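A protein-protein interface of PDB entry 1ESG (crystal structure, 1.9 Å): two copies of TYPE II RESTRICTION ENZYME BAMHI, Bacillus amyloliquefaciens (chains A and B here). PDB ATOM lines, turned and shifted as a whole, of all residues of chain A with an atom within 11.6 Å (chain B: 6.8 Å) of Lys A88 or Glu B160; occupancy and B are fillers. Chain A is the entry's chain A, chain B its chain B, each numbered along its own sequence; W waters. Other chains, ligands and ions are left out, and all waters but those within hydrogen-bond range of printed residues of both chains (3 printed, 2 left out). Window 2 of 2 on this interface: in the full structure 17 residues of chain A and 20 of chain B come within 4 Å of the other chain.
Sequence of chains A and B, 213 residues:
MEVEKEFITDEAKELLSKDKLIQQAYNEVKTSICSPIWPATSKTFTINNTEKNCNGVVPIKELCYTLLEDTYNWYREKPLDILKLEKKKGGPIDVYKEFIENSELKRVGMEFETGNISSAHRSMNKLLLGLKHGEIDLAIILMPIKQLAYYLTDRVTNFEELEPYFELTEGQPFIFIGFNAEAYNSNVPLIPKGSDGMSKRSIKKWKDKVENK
OH of Tyr B165 sits at hydrogen-bond distance from O of Lys A89 (2.7 Å). O of Lys A88 sits close to O of Glu B161 (3.4 Å).
OE2 of Glu A135 is in salt-bridge range of NZ of Lys A89, at 3.6 Å. O of Pro A92 lies within hydrogen-bond range of NZ of Lys A126. The backbone NH of Lys B146 is in hydrogen-bond range of the side-chain carboxylate of Glu B160 (2.8 Å). The side-chain amide nitrogen (ND2) of Asn B158 lies close to the backbone NH (N) of Glu B160 (3.2 Å). The side-chain amide nitrogen (ND2) of Asn B158 sits close to the backbone NH (N) of Glu B161 (3.0 Å).
Among the printed residues, merely in contact across the chains: Lys A88 with Glu B160 (3.2 Å), Lys A88 with Pro B164 (3.1 Å), Asn A125 with Tyr B165 (3.4 Å), Lys A126 with Tyr B165 (3.7 Å), Leu A129 with Pro B164 (3.7 Å) and Leu A129 with Tyr B165 (3.6 Å).
Of the printed residues of chain B, Lys A88 touches Glu B160 (3.2 Å), Glu B161 (3.4 Å) and Pro B164 (3.1 Å). Of the printed residues of chain A, Glu B160 touches Lys A88 (3.2 Å). No residue of chain A comes within 4 Å of Ile B145. No residue of chain A comes within 4 Å of Lys B146. No residue of chain A comes within 4 Å of Asn B158. Of the printed residues of chain A, Glu B161 touches Lys A88 (3.4 Å). Pro B164 touches just these residues of chain A: Lys A88 and Leu A129. Of the printed residues of chain B, Lys A126 touches Tyr B165. Of the printed residues of chain B, Lys A89 touches Tyr B165. Of the printed residues of chain A, Tyr B165 touches Lys A89 (2.7 Å), Asn A125 (3.4 Å), Lys A126 (3.7 Å) and Leu A129 (3.6 Å). Printed residues of chain B within 4 Å of Asn A125: Tyr B165 (3.4 Å). Of the printed residues of chain B, Leu A129 touches Pro B164 and Tyr B165. Glu A86 touches none of the printed residues of chain B. Phe B166 touches none of the printed residues of chain A.
Printed residues of chain A that touch a printed residue of chain B: Lys A88, Lys A89, Asn A125, Lys A126 and Leu A129. Hydrophobic or aromatic side chains of chain A within 4 Å of the printed part of chain B: Leu A129. Printed residues of chain B that touch a printed residue of chain A: Glu B160, Glu B161, Pro B164 and Tyr B165. Hydrophobic or aromatic side chains of chain B that line the printed part of chain A: Pro B164 and Tyr B165. Among the printed residues, no Asp or Glu carboxylate lies within 4 Å of a Lys or Arg side-chain nitrogen of the other chain.
No position is printed for both chains. Of the 8 pairs that touch across the chains among the printed residues, none has its exchanged pair printed and touching as well.
Water W2 bridges O of Lys A89 and OH of Tyr B165. Water W1 bridges the backbone carbonyl oxygen of Pro B164 and a ring nitrogen (NE2) of His A133. Water W3 lies within hydrogen-bond range of the side-chain amino group (NZ) of Lys A88 (3.3 Å) and the side-chain amino group (NZ) of Lys B146 (3.5 Å).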
ATOM      1  N   ILE A  82     -11.547  19.769  33.013  1.00  0.00           N
ATOM      2  CA  ILE A  82     -12.967  19.478  33.192  1.00  0.00           C
ATOM      3  C   ILE A  82     -13.531  20.313  34.340  1.00  0.00           C
ATOM      4  O   ILE A  82     -14.633  20.855  34.251  1.00  0.00           O
ATOM      5  CB  ILE A  82     -13.175  17.966  33.465  1.00  0.00           C
ATOM      6  CG1 ILE A  82     -12.680  17.165  32.255  1.00  0.00           C
ATOM      7  CG2 ILE A  82     -14.653  17.670  33.741  1.00  0.00           C
ATOM      8  CD1 ILE A  82     -12.604  15.647  32.469  1.00  0.00           C
ATOM      9  N   LEU A  83     -12.756  20.431  35.407  1.00  0.00           N
ATOM     10  CA  LEU A  83     -13.165  21.199  36.574  1.00  0.00           C
ATOM     11  C   LEU A  83     -13.490  22.661  36.239  1.00  0.00           C
ATOM     12  O   LEU A  83     -14.433  23.228  36.791  1.00  0.00           O
ATOM     13  CB  LEU A  83     -12.056  21.157  37.624  1.00  0.00           C
ATOM     14  CG  LEU A  83     -12.414  21.640  39.028  1.00  0.00           C
ATOM     15  CD1 LEU A  83     -13.382  20.645  39.667  1.00  0.00           C
ATOM     16  CD2 LEU A  83     -11.146  21.774  39.868  1.00  0.00           C
ATOM     17  N   LYS A  84     -12.732  23.275  35.334  1.00  0.00           N
ATOM     18  CA  LYS A  84     -12.992  24.675  35.006  1.00  0.00           C
ATOM     19  C   LYS A  84     -13.897  24.941  33.807  1.00  0.00           C
ATOM     20  O   LYS A  84     -14.378  26.060  33.641  1.00  0.00           O
ATOM     21  CB  LYS A  84     -11.668  25.425  34.820  1.00  0.00           C
ATOM     22  CG  LYS A  84     -10.851  25.001  33.619  1.00  0.00           C
ATOM     23  CD  LYS A  84      -9.582  25.836  33.540  1.00  0.00           C
ATOM     24  CE  LYS A  84      -8.749  25.496  32.325  1.00  0.00           C
ATOM     25  NZ  LYS A  84      -7.484  26.294  32.262  1.00  0.00           N
ATOM     26  N   LEU A  85     -14.156  23.922  32.991  1.00  0.00           N
ATOM     27  CA  LEU A  85     -14.988  24.084  31.796  1.00  0.00           C
ATOM     28  C   LEU A  85     -16.445  23.636  31.863  1.00  0.00           C
ATOM     29  O   LEU A  85     -17.054  23.426  30.817  1.00  0.00           O
ATOM     30  CB  LEU A  85     -14.358  23.345  30.618  1.00  0.00           C
ATOM     31  CG  LEU A  85     -13.016  23.780  30.054  1.00  0.00           C
ATOM     32  CD1 LEU A  85     -12.542  22.724  29.050  1.00  0.00           C
ATOM     33  CD2 LEU A  85     -13.154  25.145  29.389  1.00  0.00           C
ATOM     34  N   GLU A  86     -17.028  23.491  33.046  1.00  0.00           N
ATOM     35  CA  GLU A  86     -18.416  23.028  33.081  1.00  0.00           C
ATOM     36  C   GLU A  86     -19.441  23.988  33.679  1.00  0.00           C
ATOM     37  O   GLU A  86     -19.307  24.438  34.816  1.00  0.00           O
ATOM     38  CB  GLU A  86     -18.490  21.673  33.793  1.00  0.00           C
ATOM     39  CG  GLU A  86     -17.498  20.640  33.254  1.00  0.00           C
ATOM     40  CD  GLU A  86     -17.739  19.242  33.808  1.00  0.00           C
ATOM     41  OE1 GLU A  86     -18.181  19.128  34.970  1.00  0.00           O
ATOM     42  OE2 GLU A  86     -17.473  18.254  33.087  1.00  0.00           O
ATOM     43  N   LYS A  87     -20.469  24.292  32.891  1.00  0.00           N
ATOM     44  CA  LYS A  87     -21.548  25.189  33.303  1.00  0.00           C
ATOM     45  C   LYS A  87     -22.871  24.451  33.150  1.00  0.00           C
ATOM     46  O   LYS A  87     -23.346  23.806  34.084  1.00  0.00           O
ATOM     47  CB  LYS A  87     -21.559  26.450  32.427  1.00  0.00           C
ATOM     48  CG  LYS A  87     -22.661  27.457  32.759  1.00  0.00           C
ATOM     49  CD  LYS A  87     -22.444  28.099  34.120  1.00  0.00           C
ATOM     50  CE  LYS A  87     -23.487  29.168  34.409  1.00  0.00           C
ATOM     51  NZ  LYS A  87     -23.302  29.778  35.759  1.00  0.00           N
ATOM     52  N   LYS A  88     -23.458  24.549  31.961  1.00  0.00           N
ATOM     53  CA  LYS A  88     -24.717  23.880  31.670  1.00  0.00           C
ATOM     54  C   LYS A  88     -24.587  22.997  30.442  1.00  0.00           C
ATOM     55  O   LYS A  88     -25.579  22.458  29.950  1.00  0.00           O
ATOM     56  CB  LYS A  88     -25.833  24.906  31.461  1.00  0.00           C
ATOM     57  CG  LYS A  88     -26.714  25.099  32.682  1.00  0.00           C
ATOM     58  CD  LYS A  88     -27.500  26.387  32.592  1.00  0.00           C
ATOM     59  CE  LYS A  88     -26.571  27.582  32.667  1.00  0.00           C
ATOM     60  NZ  LYS A  88     -25.797  27.566  33.938  1.00  0.00           N
ATOM     61  N   LYS A  89     -23.364  22.852  29.943  1.00  0.00           N
ATOM     62  CA  LYS A  89     -23.139  22.012  28.777  1.00  0.00           C
ATOM     63  C   LYS A  89     -22.819  20.576  29.186  1.00  0.00           C
ATOM     64  O   LYS A  89     -23.104  19.642  28.442  1.00  0.00           O
ATOM     65  CB  LYS A  89     -22.014  22.580  27.907  1.00  0.00           C
ATOM     66  CG  LYS A  89     -22.444  23.725  27.002  1.00  0.00           C
ATOM     67  CD  LYS A  89     -21.330  24.094  26.034  1.00  0.00           C
ATOM     68  CE  LYS A  89     -21.769  25.179  25.068  1.00  0.00           C
ATOM     69  NZ  LYS A  89     -20.679  25.540  24.117  1.00  0.00           N
ATOM     70  N   GLY A  90     -22.219  20.399  30.361  1.00  0.00           N
ATOM     71  CA  GLY A  90     -21.916  19.058  30.830  1.00  0.00           C
ATOM     72  C   GLY A  90     -20.554  18.459  30.519  1.00  0.00           C
ATOM     73  O   GLY A  90     -20.456  17.280  30.180  1.00  0.00           O
ATOM     74  N   GLY A  91     -19.496  19.249  30.631  1.00  0.00           N
ATOM     75  CA  GLY A  91     -18.171  18.709  30.373  1.00  0.00           C
ATOM     76  C   GLY A  91     -17.756  18.749  28.915  1.00  0.00           C
ATOM     77  O   GLY A  91     -18.561  18.487  28.029  1.00  0.00           O
ATOM     78  N   PRO A  92     -16.490  19.067  28.641  1.00  0.00           N
ATOM     79  CA  PRO A  92     -15.983  19.139  27.271  1.00  0.00           C
ATOM     80  C   PRO A  92     -15.896  17.776  26.591  1.00  0.00           C
ATOM     81  O   PRO A  92     -16.023  16.736  27.234  1.00  0.00           O
ATOM     82  CB  PRO A  92     -14.607  19.775  27.449  1.00  0.00           C
ATOM     83  CG  PRO A  92     -14.155  19.178  28.759  1.00  0.00           C
ATOM     84  CD  PRO A  92     -15.412  19.300  29.619  1.00  0.00           C
ATOM     85  N   ILE A  93     -15.681  17.807  25.282  1.00  0.00           N
ATOM     86  CA  ILE A  93     -15.534  16.604  24.480  1.00  0.00           C
ATOM     87  C   ILE A  93     -14.264  15.933  25.008  1.00  0.00           C
ATOM     88  O   ILE A  93     -13.263  16.615  25.253  1.00  0.00           O
ATOM     89  CB  ILE A  93     -15.414  17.006  23.004  1.00  0.00           C
ATOM     90  CG1 ILE A  93     -16.793  17.496  22.518  1.00  0.00           C
ATOM     91  CG2 ILE A  93     -14.886  15.854  22.155  1.00  0.00           C
ATOM     92  CD1 ILE A  93     -16.761  18.147  21.134  1.00  0.00           C
ATOM     93  N   ARG A 122     -26.172  11.295  25.367  1.00  0.00           N
ATOM     94  CA  ARG A 122     -25.644  12.582  25.825  1.00  0.00           C
ATOM     95  C   ARG A 122     -24.363  12.922  25.089  1.00  0.00           C
ATOM     96  O   ARG A 122     -24.138  14.086  24.704  1.00  0.00           O
ATOM     97  CB  ARG A 122     -25.380  12.578  27.337  1.00  0.00           C
ATOM     98  CG  ARG A 122     -24.903  13.957  27.850  1.00  0.00           C
ATOM     99  CD  ARG A 122     -24.751  14.014  29.373  1.00  0.00           C
ATOM    100  NE  ARG A 122     -23.637  13.182  29.805  1.00  0.00           N
ATOM    101  CZ  ARG A 122     -23.291  12.970  31.070  1.00  0.00           C
ATOM    102  NH1 ARG A 122     -23.972  13.535  32.060  1.00  0.00           N
ATOM    103  NH2 ARG A 122     -22.263  12.176  31.342  1.00  0.00           N
ATOM    104  N   ASN A 125     -25.045  14.026  21.500  1.00  0.00           N
ATOM    105  CA  ASN A 125     -25.591  15.386  21.504  1.00  0.00           C
ATOM    106  C   ASN A 125     -24.508  16.435  21.849  1.00  0.00           C
ATOM    107  O   ASN A 125     -24.541  17.558  21.357  1.00  0.00           O
ATOM    108  CB  ASN A 125     -26.770  15.496  22.499  1.00  0.00           C
ATOM    109  CG  ASN A 125     -28.057  14.821  21.986  1.00  0.00           C
ATOM    110  OD1 ASN A 125     -29.073  14.747  22.706  1.00  0.00           O
ATOM    111  ND2 ASN A 125     -28.022  14.331  20.767  1.00  0.00           N
ATOM    112  N   LYS A 126     -23.564  16.067  22.707  1.00  0.00           N
ATOM    113  CA  LYS A 126     -22.447  16.951  23.074  1.00  0.00           C
ATOM    114  C   LYS A 126     -21.695  17.267  21.770  1.00  0.00           C
ATOM    115  O   LYS A 126     -21.379  18.418  21.454  1.00  0.00           O
ATOM    116  CB  LYS A 126     -21.461  16.192  23.957  1.00  0.00           C
ATOM    117  CG  LYS A 126     -21.255  16.580  25.383  1.00  0.00           C
ATOM    118  CD  LYS A 126     -19.836  16.118  25.730  1.00  0.00           C
ATOM    119  CE  LYS A 126     -19.673  15.646  27.148  1.00  0.00           C
ATOM    120  NZ  LYS A 126     -18.321  15.059  27.277  1.00  0.00           N
ATOM    121  N   LEU A 129     -23.725  19.387  19.292  1.00  0.00           N
ATOM    122  CA  LEU A 129     -23.768  20.801  19.656  1.00  0.00           C
ATOM    123  C   LEU A 129     -22.428  21.449  19.306  1.00  0.00           C
ATOM    124  O   LEU A 129     -22.388  22.603  18.888  1.00  0.00           O
ATOM    125  CB  LEU A 129     -24.066  20.984  21.156  1.00  0.00           C
ATOM    126  CG  LEU A 129     -24.420  22.405  21.614  1.00  0.00           C
ATOM    127  CD1 LEU A 129     -25.747  22.844  20.968  1.00  0.00           C
ATOM    128  CD2 LEU A 129     -24.550  22.453  23.142  1.00  0.00           C
ATOM    129  N   GLY A 130     -21.338  20.694  19.445  1.00  0.00           N
ATOM    130  CA  GLY A 130     -20.012  21.231  19.116  1.00  0.00           C
ATOM    131  C   GLY A 130     -19.881  21.509  17.631  1.00  0.00           C
ATOM    132  O   GLY A 130     -19.259  22.482  17.207  1.00  0.00           O
ATOM    133  N   HIS A 133     -21.963  24.565  16.847  1.00  0.00           N
ATOM    134  CA  HIS A 133     -21.330  25.787  17.324  1.00  0.00           C
ATOM    135  C   HIS A 133     -19.991  26.088  16.642  1.00  0.00           C
ATOM    136  O   HIS A 133     -19.326  27.063  16.982  1.00  0.00           O
ATOM    137  CB  HIS A 133     -21.152  25.715  18.839  1.00  0.00           C
ATOM    138  CG  HIS A 133     -22.434  25.887  19.600  1.00  0.00           C
ATOM    139  ND1 HIS A 133     -22.494  25.828  20.974  1.00  0.00           N
ATOM    140  CD2 HIS A 133     -23.694  26.155  19.178  1.00  0.00           C
ATOM    141  CE1 HIS A 133     -23.735  26.057  21.370  1.00  0.00           C
ATOM    142  NE2 HIS A 133     -24.484  26.258  20.301  1.00  0.00           N
ATOM    143  N   GLU A 135     -17.179  24.504  16.867  1.00  0.00           N
ATOM    144  CA  GLU A 135     -16.025  24.185  17.718  1.00  0.00           C
ATOM    145  C   GLU A 135     -15.245  22.951  17.251  1.00  0.00           C
ATOM    146  O   GLU A 135     -14.069  22.789  17.592  1.00  0.00           O
ATOM    147  CB  GLU A 135     -16.471  24.039  19.182  1.00  0.00           C
ATOM    148  CG  GLU A 135     -17.104  25.340  19.716  1.00  0.00           C
ATOM    149  CD  GLU A 135     -17.822  25.155  21.040  1.00  0.00           C
ATOM    150  OE1 GLU A 135     -18.287  24.029  21.309  1.00  0.00           O
ATOM    151  OE2 GLU A 135     -17.939  26.140  21.804  1.00  0.00           O
ATOM    152  N   LYS B   5     -40.791  28.573  32.879  1.00  0.00           N
ATOM    153  CA  LYS B   5     -39.867  28.656  31.737  1.00  0.00           C
ATOM    154  C   LYS B   5     -40.450  27.811  30.613  1.00  0.00           C
ATOM    155  O   LYS B   5     -41.085  26.784  30.855  1.00  0.00           O
ATOM    156  CB  LYS B   5     -38.488  28.084  32.090  1.00  0.00           C
ATOM    157  CG  LYS B   5     -37.804  28.740  33.264  1.00  0.00           C
ATOM    158  CD  LYS B   5     -37.495  30.192  32.989  1.00  0.00           C
ATOM    159  CE  LYS B   5     -36.684  30.775  34.151  1.00  0.00           C
ATOM    160  NZ  LYS B   5     -36.360  32.200  33.922  1.00  0.00           N
ATOM    161  N   MET B 143     -40.091  19.366  32.580  1.00  0.00           N
ATOM    162  CA  MET B 143     -39.004  19.205  33.543  1.00  0.00           C
ATOM    163  C   MET B 143     -39.142  20.216  34.666  1.00  0.00           C
ATOM    164  O   MET B 143     -39.687  21.286  34.471  1.00  0.00           O
ATOM    165  CB  MET B 143     -37.644  19.487  32.887  1.00  0.00           C
ATOM    166  CG  MET B 143     -37.296  18.654  31.692  1.00  0.00           C
ATOM    167  SD  MET B 143     -35.729  19.248  30.947  1.00  0.00           S
ATOM    168  CE  MET B 143     -35.095  17.713  30.388  1.00  0.00           C
ATOM    169  N   PRO B 144     -38.637  19.890  35.857  1.00  0.00           N
ATOM    170  CA  PRO B 144     -38.749  20.886  36.921  1.00  0.00           C
ATOM    171  C   PRO B 144     -37.653  21.928  36.648  1.00  0.00           C
ATOM    172  O   PRO B 144     -36.603  21.597  36.061  1.00  0.00           O
ATOM    173  CB  PRO B 144     -38.440  20.083  38.178  1.00  0.00           C
ATOM    174  CG  PRO B 144     -37.491  18.998  37.657  1.00  0.00           C
ATOM    175  CD  PRO B 144     -38.122  18.602  36.367  1.00  0.00           C
ATOM    176  N   ILE B 145     -37.884  23.185  37.009  1.00  0.00           N
ATOM    177  CA  ILE B 145     -36.800  24.148  36.832  1.00  0.00           C
ATOM    178  C   ILE B 145     -35.804  23.904  37.969  1.00  0.00           C
ATOM    179  O   ILE B 145     -36.123  23.232  38.956  1.00  0.00           O
ATOM    180  CB  ILE B 145     -37.281  25.631  36.835  1.00  0.00           C
ATOM    181  CG1 ILE B 145     -37.895  26.005  38.185  1.00  0.00           C
ATOM    182  CG2 ILE B 145     -38.259  25.852  35.690  1.00  0.00           C
ATOM    183  CD1 ILE B 145     -38.213  27.499  38.290  1.00  0.00           C
ATOM    184  N   LYS B 146     -34.598  24.443  37.821  1.00  0.00           N
ATOM    185  CA  LYS B 146     -33.518  24.251  38.775  1.00  0.00           C
ATOM    186  C   LYS B 146     -33.847  24.566  40.234  1.00  0.00           C
ATOM    187  O   LYS B 146     -33.469  23.823  41.133  1.00  0.00           O
ATOM    188  CB  LYS B 146     -32.316  25.089  38.324  1.00  0.00           C
ATOM    189  CG  LYS B 146     -31.090  24.959  39.197  1.00  0.00           C
ATOM    190  CD  LYS B 146     -29.973  25.827  38.643  1.00  0.00           C
ATOM    191  CE  LYS B 146     -28.800  25.891  39.603  1.00  0.00           C
ATOM    192  NZ  LYS B 146     -27.809  26.913  39.180  1.00  0.00           N
ATOM    193  N   GLN B 147     -34.544  25.667  40.473  1.00  0.00           N
ATOM    194  CA  GLN B 147     -34.871  26.039  41.845  1.00  0.00           C
ATOM    195  C   GLN B 147     -35.656  24.924  42.550  1.00  0.00           C
ATOM    196  O   GLN B 147     -35.420  24.621  43.721  1.00  0.00           O
ATOM    197  CB  GLN B 147     -35.678  27.342  41.873  1.00  0.00           C
ATOM    198  CG  GLN B 147     -36.009  27.779  43.311  1.00  0.00           C
ATOM    199  CD  GLN B 147     -37.042  28.891  43.381  1.00  0.00           C
ATOM    200  OE1 GLN B 147     -37.776  29.129  42.434  1.00  0.00           O
ATOM    201  NE2 GLN B 147     -37.109  29.560  44.522  1.00  0.00           N
ATOM    202  N   THR B 157     -33.019  15.591  36.311  1.00  0.00           N
ATOM    203  CA  THR B 157     -32.872  16.577  35.232  1.00  0.00           C
ATOM    204  C   THR B 157     -33.595  17.883  35.606  1.00  0.00           C
ATOM    205  O   THR B 157     -34.648  17.837  36.235  1.00  0.00           O
ATOM    206  CB  THR B 157     -33.559  16.083  33.920  1.00  0.00           C
ATOM    207  OG1 THR B 157     -33.007  14.836  33.497  1.00  0.00           O
ATOM    208  CG2 THR B 157     -33.382  17.102  32.809  1.00  0.00           C
ATOM    209  N   ASN B 158     -33.034  19.036  35.257  1.00  0.00           N
ATOM    210  CA  ASN B 158     -33.759  20.293  35.471  1.00  0.00           C
ATOM    211  C   ASN B 158     -33.731  21.058  34.152  1.00  0.00           C
ATOM    212  O   ASN B 158     -32.838  20.848  33.313  1.00  0.00           O
ATOM    213  CB  ASN B 158     -33.240  21.137  36.666  1.00  0.00           C
ATOM    214  CG  ASN B 158     -31.835  21.648  36.487  1.00  0.00           C
ATOM    215  OD1 ASN B 158     -30.913  21.220  37.185  1.00  0.00           O
ATOM    216  ND2 ASN B 158     -31.665  22.587  35.581  1.00  0.00           N
ATOM    217  N   PHE B 159     -34.720  21.923  33.961  1.00  0.00           N
ATOM    218  CA  PHE B 159     -34.883  22.687  32.718  1.00  0.00           C
ATOM    219  C   PHE B 159     -33.609  23.343  32.216  1.00  0.00           C
ATOM    220  O   PHE B 159     -33.218  23.159  31.059  1.00  0.00           O
ATOM    221  CB  PHE B 159     -35.963  23.767  32.905  1.00  0.00           C
ATOM    222  CG  PHE B 159     -36.325  24.531  31.640  1.00  0.00           C
ATOM    223  CD1 PHE B 159     -35.609  25.662  31.253  1.00  0.00           C
ATOM    224  CD2 PHE B 159     -37.422  24.152  30.879  1.00  0.00           C
ATOM    225  CE1 PHE B 159     -35.986  26.413  30.119  1.00  0.00           C
ATOM    226  CE2 PHE B 159     -37.812  24.888  29.743  1.00  0.00           C
ATOM    227  CZ  PHE B 159     -37.089  26.027  29.364  1.00  0.00           C
ATOM    228  N   GLU B 160     -32.973  24.107  33.093  1.00  0.00           N
ATOM    229  CA  GLU B 160     -31.765  24.831  32.722  1.00  0.00           C
ATOM    230  C   GLU B 160     -30.602  23.932  32.309  1.00  0.00           C
ATOM    231  O   GLU B 160     -29.719  24.366  31.577  1.00  0.00           O
ATOM    232  CB  GLU B 160     -31.313  25.740  33.880  1.00  0.00           C
ATOM    233  CG  GLU B 160     -32.247  26.927  34.184  1.00  0.00           C
ATOM    234  CD  GLU B 160     -33.378  26.598  35.194  1.00  0.00           C
ATOM    235  OE1 GLU B 160     -33.893  27.542  35.816  1.00  0.00           O
ATOM    236  OE2 GLU B 160     -33.764  25.421  35.362  1.00  0.00           O
ATOM    237  N   GLU B 161     -30.589  22.698  32.781  1.00  0.00           N
ATOM    238  CA  GLU B 161     -29.484  21.808  32.422  1.00  0.00           C
ATOM    239  C   GLU B 161     -29.617  21.288  30.996  1.00  0.00           C
ATOM    240  O   GLU B 161     -28.615  21.074  30.317  1.00  0.00           O
ATOM    241  CB  GLU B 161     -29.380  20.642  33.410  1.00  0.00           C
ATOM    242  CG  GLU B 161     -28.098  19.862  33.268  1.00  0.00           C
ATOM    243  CD  GLU B 161     -27.784  18.992  34.470  1.00  0.00           C
ATOM    244  OE1 GLU B 161     -26.679  18.412  34.488  1.00  0.00           O
ATOM    245  OE2 GLU B 161     -28.625  18.884  35.392  1.00  0.00           O
ATOM    246  N   LEU B 162     -30.846  21.085  30.530  1.00  0.00           N
ATOM    247  CA  LEU B 162     -31.031  20.615  29.169  1.00  0.00           C
ATOM    248  C   LEU B 162     -31.093  21.788  28.179  1.00  0.00           C
ATOM    249  O   LEU B 162     -30.827  21.606  27.004  1.00  0.00           O
ATOM    250  CB  LEU B 162     -32.314  19.775  29.051  1.00  0.00           C
ATOM    251  CG  LEU B 162     -32.555  19.107  27.691  1.00  0.00           C
ATOM    252  CD1 LEU B 162     -31.388  18.133  27.393  1.00  0.00           C
ATOM    253  CD2 LEU B 162     -33.893  18.332  27.691  1.00  0.00           C
ATOM    254  N   GLU B 163     -31.390  22.990  28.677  1.00  0.00           N
ATOM    255  CA  GLU B 163     -31.535  24.179  27.841  1.00  0.00           C
ATOM    256  C   GLU B 163     -30.448  24.451  26.775  1.00  0.00           C
ATOM    257  O   GLU B 163     -30.764  24.842  25.667  1.00  0.00           O
ATOM    258  CB  GLU B 163     -31.726  25.418  28.742  1.00  0.00           C
ATOM    259  CG  GLU B 163     -32.175  26.668  27.988  1.00  0.00           C
ATOM    260  CD  GLU B 163     -32.534  27.833  28.920  1.00  0.00           C
ATOM    261  OE1 GLU B 163     -32.014  27.893  30.058  1.00  0.00           O
ATOM    262  OE2 GLU B 163     -33.334  28.699  28.502  1.00  0.00           O
ATOM    263  N   PRO B 164     -29.162  24.239  27.090  1.00  0.00           N
ATOM    264  CA  PRO B 164     -28.130  24.493  26.069  1.00  0.00           C
ATOM    265  C   PRO B 164     -28.332  23.624  24.825  1.00  0.00           C
ATOM    266  O   PRO B 164     -27.876  23.958  23.728  1.00  0.00           O
ATOM    267  CB  PRO B 164     -26.827  24.136  26.796  1.00  0.00           C
ATOM    268  CG  PRO B 164     -27.145  24.448  28.234  1.00  0.00           C
ATOM    269  CD  PRO B 164     -28.555  23.874  28.374  1.00  0.00           C
ATOM    270  N   TYR B 165     -29.037  22.508  25.007  1.00  0.00           N
ATOM    271  CA  TYR B 165     -29.285  21.561  23.916  1.00  0.00           C
ATOM    272  C   TYR B 165     -30.617  21.716  23.187  1.00  0.00           C
ATOM    273  O   TYR B 165     -30.887  20.990  22.232  1.00  0.00           O
ATOM    274  CB  TYR B 165     -29.149  20.126  24.448  1.00  0.00           C
ATOM    275  CG  TYR B 165     -27.728  19.813  24.848  1.00  0.00           C
ATOM    276  CD1 TYR B 165     -26.809  19.348  23.906  1.00  0.00           C
ATOM    277  CD2 TYR B 165     -27.278  20.069  26.145  1.00  0.00           C
ATOM    278  CE1 TYR B 165     -25.471  19.153  24.237  1.00  0.00           C
ATOM    279  CE2 TYR B 165     -25.941  19.877  26.493  1.00  0.00           C
ATOM    280  CZ  TYR B 165     -25.044  19.420  25.529  1.00  0.00           C
ATOM    281  OH  TYR B 165     -23.717  19.237  25.850  1.00  0.00           O
ATOM    282  N   PHE B 166     -31.459  22.649  23.623  1.00  0.00           N
ATOM    283  CA  PHE B 166     -32.733  22.848  22.927  1.00  0.00           C
ATOM    284  C   PHE B 166     -32.476  23.156  21.456  1.00  0.00           C
ATOM    285  O   PHE B 166     -33.282  22.804  20.598  1.00  0.00           O
ATOM    286  CB  PHE B 166     -33.506  24.040  23.482  1.00  0.00           C
ATOM    287  CG  PHE B 166     -34.039  23.842  24.863  1.00  0.00           C
ATOM    288  CD1 PHE B 166     -33.995  22.604  25.489  1.00  0.00           C
ATOM    289  CD2 PHE B 166     -34.579  24.937  25.548  1.00  0.00           C
ATOM    290  CE1 PHE B 166     -34.484  22.450  26.795  1.00  0.00           C
ATOM    291  CE2 PHE B 166     -35.068  24.798  26.842  1.00  0.00           C
ATOM    292  CZ  PHE B 166     -35.019  23.561  27.466  1.00  0.00           C
HETATM  293  O   HOH W   1     -25.983  25.955  23.438  1.00  0.00           O
HETATM  294  O   HOH W   2     -23.546  17.052  27.792  1.00  0.00           O
HETATM  295  O   HOH W   3     -28.518  27.214  35.768  1.00  0.00           O
